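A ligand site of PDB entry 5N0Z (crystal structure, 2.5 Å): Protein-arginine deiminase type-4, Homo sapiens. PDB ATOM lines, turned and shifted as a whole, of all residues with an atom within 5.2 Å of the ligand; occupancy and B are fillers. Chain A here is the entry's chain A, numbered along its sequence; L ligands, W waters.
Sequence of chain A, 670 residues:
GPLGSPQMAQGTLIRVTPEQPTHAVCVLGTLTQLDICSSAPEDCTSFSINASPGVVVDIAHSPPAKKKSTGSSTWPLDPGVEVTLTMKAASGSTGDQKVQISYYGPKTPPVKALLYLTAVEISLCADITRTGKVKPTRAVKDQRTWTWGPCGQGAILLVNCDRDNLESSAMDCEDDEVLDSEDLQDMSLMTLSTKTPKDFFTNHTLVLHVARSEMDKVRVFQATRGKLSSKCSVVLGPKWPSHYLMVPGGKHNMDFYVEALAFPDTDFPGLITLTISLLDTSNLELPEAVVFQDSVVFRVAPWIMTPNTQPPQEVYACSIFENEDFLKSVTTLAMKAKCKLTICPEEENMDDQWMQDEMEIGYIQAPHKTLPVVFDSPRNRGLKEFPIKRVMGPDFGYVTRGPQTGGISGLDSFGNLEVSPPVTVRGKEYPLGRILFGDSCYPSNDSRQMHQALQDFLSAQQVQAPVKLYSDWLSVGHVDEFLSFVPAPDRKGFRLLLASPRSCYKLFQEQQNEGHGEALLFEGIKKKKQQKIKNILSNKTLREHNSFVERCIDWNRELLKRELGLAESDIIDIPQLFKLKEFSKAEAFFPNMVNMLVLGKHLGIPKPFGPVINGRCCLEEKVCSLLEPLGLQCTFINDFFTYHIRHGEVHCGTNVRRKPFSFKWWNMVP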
ATOM      1  N   ASP A 351       2.030  20.787  10.874  1.00  0.00           N
ATOM      2  CA  ASP A 351       3.473  20.540  10.635  1.00  0.00           C
ATOM      3  C   ASP A 351       3.793  19.133  10.126  1.00  0.00           C
ATOM      4  O   ASP A 351       4.948  18.844   9.818  1.00  0.00           O
ATOM      5  CB  ASP A 351       4.367  20.827  11.897  1.00  0.00           C
ATOM      6  CG  ASP A 351       4.989  22.206  11.901  1.00  0.00           C
ATOM      7  OD1 ASP A 351       4.540  23.094  11.135  1.00  0.00           O
ATOM      8  OD2 ASP A 351       5.945  22.413  12.688  1.00  0.00           O
ATOM      9  N   GLN A 353       4.137  16.530   7.550  1.00  0.00           N
ATOM     10  CA  GLN A 353       4.285  16.510   6.093  1.00  0.00           C
ATOM     11  C   GLN A 353       4.203  15.107   5.506  1.00  0.00           C
ATOM     12  O   GLN A 353       4.130  14.956   4.243  1.00  0.00           O
ATOM     13  CB  GLN A 353       5.591  17.180   5.666  1.00  0.00           C
ATOM     14  CG  GLN A 353       6.846  16.329   5.847  1.00  0.00           C
ATOM     15  CD  GLN A 353       8.102  17.153   6.044  1.00  0.00           C
ATOM     16  OE1 GLN A 353       8.301  17.800   7.075  1.00  0.00           O
ATOM     17  NE2 GLN A 353       8.968  17.133   5.042  1.00  0.00           N
ATOM     18  N   TRP A 354       4.199  14.106   6.403  1.00  0.00           N
ATOM     19  CA  TRP A 354       4.348  12.685   6.035  1.00  0.00           C
ATOM     20  C   TRP A 354       2.997  12.029   5.768  1.00  0.00           C
ATOM     21  O   TRP A 354       2.520  11.255   6.578  1.00  0.00           O
ATOM     22  CB  TRP A 354       5.133  11.922   7.118  1.00  0.00           C
ATOM     23  CG  TRP A 354       6.389  12.617   7.473  1.00  0.00           C
ATOM     24  CD1 TRP A 354       6.656  13.273   8.633  1.00  0.00           C
ATOM     25  CD2 TRP A 354       7.547  12.788   6.639  1.00  0.00           C
ATOM     26  NE1 TRP A 354       7.919  13.833   8.593  1.00  0.00           N
ATOM     27  CE2 TRP A 354       8.492  13.541   7.375  1.00  0.00           C
ATOM     28  CE3 TRP A 354       7.893  12.352   5.351  1.00  0.00           C
ATOM     29  CZ2 TRP A 354       9.752  13.864   6.867  1.00  0.00           C
ATOM     30  CZ3 TRP A 354       9.142  12.689   4.843  1.00  0.00           C
ATOM     31  CH2 TRP A 354      10.067  13.444   5.601  1.00  0.00           C
ATOM     32  N   GLN A 356       2.265   9.700   3.755  1.00  0.00           N
ATOM     33  CA  GLN A 356       2.424   8.256   3.640  1.00  0.00           C
ATOM     34  C   GLN A 356       2.098   7.532   4.930  1.00  0.00           C
ATOM     35  O   GLN A 356       1.548   6.447   4.910  1.00  0.00           O
ATOM     36  CB  GLN A 356       3.868   7.902   3.255  1.00  0.00           C
ATOM     37  CG  GLN A 356       4.231   6.407   3.214  1.00  0.00           C
ATOM     38  CD  GLN A 356       3.484   5.610   2.155  1.00  0.00           C
ATOM     39  OE1 GLN A 356       3.408   4.396   2.245  1.00  0.00           O
ATOM     40  NE2 GLN A 356       2.970   6.272   1.141  1.00  0.00           N
ATOM     41  N   ASP A 357       2.451   8.130   6.042  1.00  0.00           N
ATOM     42  CA  ASP A 357       2.559   7.396   7.262  1.00  0.00           C
ATOM     43  C   ASP A 357       1.295   7.289   8.059  1.00  0.00           C
ATOM     44  O   ASP A 357       1.167   6.339   8.812  1.00  0.00           O
ATOM     45  CB  ASP A 357       3.669   7.990   8.119  1.00  0.00           C
ATOM     46  CG  ASP A 357       5.038   7.821   7.496  1.00  0.00           C
ATOM     47  OD1 ASP A 357       5.199   6.962   6.581  1.00  0.00           O
ATOM     48  OD2 ASP A 357       5.957   8.561   7.940  1.00  0.00           O
ATOM     49  N   ARG A 379      -0.651   5.935  14.487  1.00  0.00           N
ATOM     50  CA  ARG A 379       0.464   6.877  14.560  1.00  0.00           C
ATOM     51  C   ARG A 379       0.045   8.141  15.297  1.00  0.00           C
ATOM     52  O   ARG A 379       0.683   8.513  16.283  1.00  0.00           O
ATOM     53  CB  ARG A 379       0.972   7.182  13.139  1.00  0.00           C
ATOM     54  CG  ARG A 379       2.205   8.068  13.008  1.00  0.00           C
ATOM     55  CD  ARG A 379       2.483   8.263  11.528  1.00  0.00           C
ATOM     56  NE  ARG A 379       3.373   9.400  11.170  1.00  0.00           N
ATOM     57  CZ  ARG A 379       2.975  10.570  10.656  1.00  0.00           C
ATOM     58  NH1 ARG A 379       3.886  11.483  10.356  1.00  0.00           N
ATOM     59  NH2 ARG A 379       1.704  10.867  10.439  1.00  0.00           N
ATOM     60  N   ARG A 381      -0.022  11.535  14.827  1.00  0.00           N
ATOM     61  CA  ARG A 381       0.711  12.801  14.856  1.00  0.00           C
ATOM     62  C   ARG A 381      -0.171  13.897  14.257  1.00  0.00           C
ATOM     63  O   ARG A 381      -1.402  13.747  14.206  1.00  0.00           O
ATOM     64  CB  ARG A 381       2.038  12.652  14.121  1.00  0.00           C
ATOM     65  CG  ARG A 381       2.948  11.671  14.823  1.00  0.00           C
ATOM     66  CD  ARG A 381       4.413  11.930  14.543  1.00  0.00           C
ATOM     67  NE  ARG A 381       5.212  11.240  15.541  1.00  0.00           N
ATOM     68  CZ  ARG A 381       6.515  11.460  15.761  1.00  0.00           C
ATOM     69  NH1 ARG A 381       7.134  10.763  16.722  1.00  0.00           N
ATOM     70  NH2 ARG A 381       7.202  12.339  15.039  1.00  0.00           N
ATOM     71  N   GLY A 410       7.459   3.575  15.546  1.00  0.00           N
ATOM     72  CA  GLY A 410       7.619   4.048  14.176  1.00  0.00           C
ATOM     73  C   GLY A 410       7.185   3.013  13.160  1.00  0.00           C
ATOM     74  O   GLY A 410       6.594   3.327  12.129  1.00  0.00           O
ATOM     75  N   SER A 413       3.806   3.140  11.383  1.00  0.00           N
ATOM     76  CA  SER A 413       3.545   4.101  10.326  1.00  0.00           C
ATOM     77  C   SER A 413       3.405   3.385   9.005  1.00  0.00           C
ATOM     78  O   SER A 413       4.092   2.427   8.729  1.00  0.00           O
ATOM     79  CB  SER A 413       4.686   5.104  10.219  1.00  0.00           C
ATOM     80  OG  SER A 413       4.748   5.905  11.384  1.00  0.00           O
ATOM     81  N   GLY A 415       4.206   3.942   6.032  1.00  0.00           N
ATOM     82  CA  GLY A 415       5.327   3.772   5.153  1.00  0.00           C
ATOM     83  C   GLY A 415       5.908   2.392   5.335  1.00  0.00           C
ATOM     84  O   GLY A 415       6.714   1.931   4.500  1.00  0.00           O
ATOM     85  N   VAL A 476      14.409   4.860  10.640  1.00  0.00           N
ATOM     86  CA  VAL A 476      12.960   5.102  10.609  1.00  0.00           C
ATOM     87  C   VAL A 476      12.181   3.772  10.680  1.00  0.00           C
ATOM     88  O   VAL A 476      11.117   3.709  11.276  1.00  0.00           O
ATOM     89  CB  VAL A 476      12.553   5.926   9.326  1.00  0.00           C
ATOM     90  CG1 VAL A 476      11.062   5.796   8.936  1.00  0.00           C
ATOM     91  CG2 VAL A 476      12.894   7.389   9.522  1.00  0.00           C
ATOM     92  N   HIS A 478      11.163   1.585   7.884  1.00  0.00           N
ATOM     93  CA  HIS A 478      10.065   1.291   6.962  1.00  0.00           C
ATOM     94  C   HIS A 478      10.487   0.581   5.713  1.00  0.00           C
ATOM     95  O   HIS A 478      11.448   1.001   5.071  1.00  0.00           O
ATOM     96  CB  HIS A 478       9.397   2.552   6.505  1.00  0.00           C
ATOM     97  CG  HIS A 478       8.713   3.287   7.593  1.00  0.00           C
ATOM     98  ND1 HIS A 478       7.947   4.398   7.343  1.00  0.00           N
ATOM     99  CD2 HIS A 478       8.678   3.086   8.930  1.00  0.00           C
ATOM    100  CE1 HIS A 478       7.470   4.857   8.484  1.00  0.00           C
ATOM    101  NE2 HIS A 478       7.886   4.067   9.464  1.00  0.00           N
ATOM    102  N   ASP A 480       9.322   0.786   2.805  1.00  0.00           N
ATOM    103  CA  ASP A 480       9.389   1.680   1.649  1.00  0.00           C
ATOM    104  C   ASP A 480      10.787   2.311   1.524  1.00  0.00           C
ATOM    105  O   ASP A 480      11.159   2.740   0.470  1.00  0.00           O
ATOM    106  CB  ASP A 480       8.235   2.720   1.620  1.00  0.00           C
ATOM    107  CG  ASP A 480       8.395   3.884   2.648  1.00  0.00           C
ATOM    108  OD1 ASP A 480       9.297   3.814   3.530  1.00  0.00           O
ATOM    109  OD2 ASP A 480       7.579   4.870   2.550  1.00  0.00           O
ATOM    110  N   GLU A 481      11.561   2.296   2.596  1.00  0.00           N
ATOM    111  CA  GLU A 481      12.922   2.776   2.527  1.00  0.00           C
ATOM    112  C   GLU A 481      13.883   1.844   1.771  1.00  0.00           C
ATOM    113  O   GLU A 481      14.980   2.280   1.429  1.00  0.00           O
ATOM    114  CB  GLU A 481      13.489   3.006   3.912  1.00  0.00           C
ATOM    115  CG  GLU A 481      12.706   3.959   4.770  1.00  0.00           C
ATOM    116  CD  GLU A 481      13.375   4.182   6.105  1.00  0.00           C
ATOM    117  OE1 GLU A 481      14.297   5.036   6.168  1.00  0.00           O
ATOM    118  OE2 GLU A 481      12.988   3.494   7.086  1.00  0.00           O
ATOM    119  N   ASN A 595      12.486   5.279  -2.645  1.00  0.00           N
ATOM    120  CA  ASN A 595      11.327   5.868  -1.948  1.00  0.00           C
ATOM    121  C   ASN A 595      10.658   6.880  -2.902  1.00  0.00           C
ATOM    122  O   ASN A 595      10.570   8.087  -2.609  1.00  0.00           O
ATOM    123  CB  ASN A 595      11.815   6.519  -0.646  1.00  0.00           C
ATOM    124  CG  ASN A 595      10.706   6.878   0.286  1.00  0.00           C
ATOM    125  OD1 ASN A 595      10.292   8.050   0.369  1.00  0.00           O
ATOM    126  ND2 ASN A 595      10.190   5.896   0.978  1.00  0.00           N
ATOM    127  N   ILE A 645      16.446  15.870   4.558  1.00  0.00           N
ATOM    128  CA  ILE A 645      17.143  16.224   5.813  1.00  0.00           C
ATOM    129  C   ILE A 645      16.261  15.966   7.030  1.00  0.00           C
ATOM    130  O   ILE A 645      16.745  16.040   8.159  1.00  0.00           O
ATOM    131  CB  ILE A 645      17.665  17.705   5.840  1.00  0.00           C
ATOM    132  CG1 ILE A 645      16.502  18.740   5.774  1.00  0.00           C
ATOM    133  CG2 ILE A 645      18.699  17.932   4.740  1.00  0.00           C
ATOM    134  CD1 ILE A 645      16.838  20.103   6.365  1.00  0.00           C
ATOM    135  N   ARG A 646      14.972  15.714   6.785  1.00  0.00           N
ATOM    136  CA  ARG A 646      14.021  15.254   7.800  1.00  0.00           C
ATOM    137  C   ARG A 646      13.814  13.730   7.798  1.00  0.00           C
ATOM    138  O   ARG A 646      12.914  13.197   8.473  1.00  0.00           O
ATOM    139  CB  ARG A 646      12.696  15.998   7.624  1.00  0.00           C
ATOM    140  CG  ARG A 646      12.736  17.418   8.141  1.00  0.00           C
ATOM    141  CD  ARG A 646      11.754  18.315   7.425  1.00  0.00           C
ATOM    142  NE  ARG A 646      11.389  19.415   8.289  1.00  0.00           N
ATOM    143  CZ  ARG A 646      10.689  20.479   7.915  1.00  0.00           C
ATOM    144  NH1 ARG A 646      10.273  20.652   6.652  1.00  0.00           N
ATOM    145  NH2 ARG A 646      10.421  21.398   8.835  1.00  0.00           N
ATOM    146  N   HIS A 647      14.672  13.029   7.063  1.00  0.00           N
ATOM    147  CA  HIS A 647      14.850  11.577   7.139  1.00  0.00           C
ATOM    148  C   HIS A 647      13.787  10.801   6.308  1.00  0.00           C
ATOM    149  O   HIS A 647      13.517   9.599   6.540  1.00  0.00           O
ATOM    150  CB  HIS A 647      14.951  11.092   8.608  1.00  0.00           C
ATOM    151  CG  HIS A 647      16.067  11.744   9.378  1.00  0.00           C
ATOM    152  ND1 HIS A 647      15.908  12.212  10.669  1.00  0.00           N
ATOM    153  CD2 HIS A 647      17.353  11.990   9.040  1.00  0.00           C
ATOM    154  CE1 HIS A 647      17.051  12.719  11.093  1.00  0.00           C
ATOM    155  NE2 HIS A 647      17.947  12.592  10.131  1.00  0.00           N
ATOM    156  N   GLY A 648      13.250  11.482   5.289  1.00  0.00           N
ATOM    157  CA  GLY A 648      12.252  10.874   4.402  1.00  0.00           C
ATOM    158  C   GLY A 648      12.311  11.467   3.014  1.00  0.00           C
ATOM    159  O   GLY A 648      12.960  12.474   2.821  1.00  0.00           O
ATOM    160  N   GLU A 649      11.647  10.841   2.041  1.00  0.00           N
ATOM    161  CA  GLU A 649      11.653  11.343   0.659  1.00  0.00           C
ATOM    162  C   GLU A 649      10.234  11.545   0.064  1.00  0.00           C
ATOM    163  O   GLU A 649       9.262  11.749   0.812  1.00  0.00           O
ATOM    164  CB  GLU A 649      12.494  10.420  -0.232  1.00  0.00           C
ATOM    165  CG  GLU A 649      13.827   9.969   0.341  1.00  0.00           C
ATOM    166  CD  GLU A 649      14.800  11.115   0.608  1.00  0.00           C
ATOM    167  OE1 GLU A 649      15.743  10.934   1.417  1.00  0.00           O
ATOM    168  OE2 GLU A 649      14.643  12.194   0.023  1.00  0.00           O
ATOM    169  N   CYS A 652       7.575   8.974   1.079  1.00  0.00           N
ATOM    170  CA  CYS A 652       7.250   9.281   2.476  1.00  0.00           C
ATOM    171  C   CYS A 652       6.318  10.499   2.683  1.00  0.00           C
ATOM    172  O   CYS A 652       5.637  10.584   3.712  1.00  0.00           O
ATOM    173  CB  CYS A 652       8.537   9.496   3.285  1.00  0.00           C
ATOM    174  SG  CYS A 652       9.712   8.114   3.419  1.00  0.00           S
HETATM  175  C1  LIG L   1      13.663  15.277  12.104  1.00  0.00           C
HETATM  176  C2  LIG L   1      10.335   8.070  14.711  1.00  0.00           C
HETATM  177  C3  LIG L   1      12.766  14.290  11.723  1.00  0.00           C
HETATM  178  C4  LIG L   1      13.286  16.599  12.144  1.00  0.00           C
HETATM  179  C5  LIG L   1      11.168   8.700  13.818  1.00  0.00           C
HETATM  180  C6  LIG L   1       8.955   8.117  14.614  1.00  0.00           C
HETATM  181  C7  LIG L   1      11.094  15.953  11.429  1.00  0.00           C
HETATM  182  C8  LIG L   1      11.463  14.617  11.374  1.00  0.00           C
HETATM  183  C9  LIG L   1      11.992  16.927  11.795  1.00  0.00           C
HETATM  184  C10 LIG L   1       9.119   9.446  12.689  1.00  0.00           C
HETATM  185  C11 LIG L   1      10.500   9.381  12.827  1.00  0.00           C
HETATM  186  C12 LIG L   1       8.306   8.816  13.596  1.00  0.00           C
HETATM  187  C13 LIG L   1       9.871  10.591  11.060  1.00  0.00           C
HETATM  188  C14 LIG L   1       9.819  16.614  11.117  1.00  0.00           C
HETATM  189  C15 LIG L   1      10.504  13.545  11.007  1.00  0.00           C
HETATM  190  C16 LIG L   1       8.452   7.300   5.588  1.00  0.00           C
HETATM  191  C17 LIG L   1      11.351  18.279  11.773  1.00  0.00           C
HETATM  192  C18 LIG L   1       9.745   7.204   4.779  1.00  0.00           C
HETATM  193  C19 LIG L   1       8.936  20.091  12.045  1.00  0.00           C
HETATM  194  C20 LIG L   1      12.374  10.306  11.522  1.00  0.00           C
HETATM  195  C21 LIG L   1       6.115   8.222  14.299  1.00  0.00           C
HETATM  196  C22 LIG L   1       9.029   9.936   8.153  1.00  0.00           C
HETATM  197  C23 LIG L   1      10.273  10.631   8.651  1.00  0.00           C
HETATM  198  C24 LIG L   1       9.034  18.955  11.056  1.00  0.00           C
HETATM  199  C25 LIG L   1       9.362   9.211   6.882  1.00  0.00           C
HETATM  200  C26 LIG L   1       9.932  11.446   9.859  1.00  0.00           C
HETATM  201  N1  LIG L   1       8.738  10.191  11.605  1.00  0.00           N
HETATM  202  N2  LIG L   1       7.452   6.545   5.291  1.00  0.00           N
HETATM  203  N3  LIG L   1      10.953  10.118  11.772  1.00  0.00           N
HETATM  204  N4  LIG L   1       9.970  17.936  11.491  1.00  0.00           N
HETATM  205  N5  LIG L   1      10.847  12.578  10.069  1.00  0.00           N
HETATM  206  N6  LIG L   1       8.356   8.195   6.633  1.00  0.00           N
HETATM  207  O1  LIG L   1       8.851  16.078  10.577  1.00  0.00           O
HETATM  208  O2  LIG L   1       9.432  13.553  11.595  1.00  0.00           O
HETATM  209  O3  LIG L   1       6.930   8.946  13.378  1.00  0.00           O
HETATM  210  O   HOH W   1       9.564   5.769  12.254  1.00  0.00           O
HETATM  211  O   HOH W   2       6.601  16.998   8.789  1.00  0.00           O
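A ring nitrogen (ND1) of His 478 lies within hydrogen-bond range of a nitrogen (N2) of the ligand, 3.0 Å away. OD1 of Asp 357 is in salt-bridge range of N2 of the ligand, 2.6 Å away. N2 of the ligand lies within salt-bridge range of OD2 of Asp 480 (3.2 Å). C18 of the ligand is bonded to SG of Cys 652 (1.6 Å). N5 of the ligand sits at hydrogen-bond distance from O of Arg 646. The indole nitrogen of Trp 354 sits at hydrogen-bond distance from an oxygen (O1) of the ligand.
Merely in contact with the ligand: Asp 351 (3.8 Å), Gln 353 (3.9 Å), Gln 356 (3.8 Å), Arg 381 (3.4 Å), Ser 413 (3.97 Å), Gly 415 (3.5 Å), Val 476 (3.6 Å) and His 647 (3.9 Å). Of the 21 residues printed, 14 come within 4 Å of the ligand.
OD1 of Asp 357 is in hydrogen-bond range of N of Gly 415 (3.2 Å). The backbone carbonyl oxygen of Cys 652 lies close to the backbone NH of Gln 356 (3.5 Å). OD1 of Asn 595 sits at hydrogen-bond distance from N of Cys 652 (3.0 Å). O of Gly 410 lies close to OG of Ser 413. OD2 of Asp 480 lies close to ND2 of Asn 595 (3.2 Å). OE2 of Glu 481 is in hydrogen-bond range of N of His 478 (2.8 Å). The guanidinium group (NH1) of Arg 646 lies within hydrogen-bond range of the side-chain amide oxygen (OE1) of Gln 353 (3.5 Å). A ring nitrogen (NE2) of His 478 is in hydrogen-bond range of the backbone carbonyl oxygen of Gly 410 (3.1 Å).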
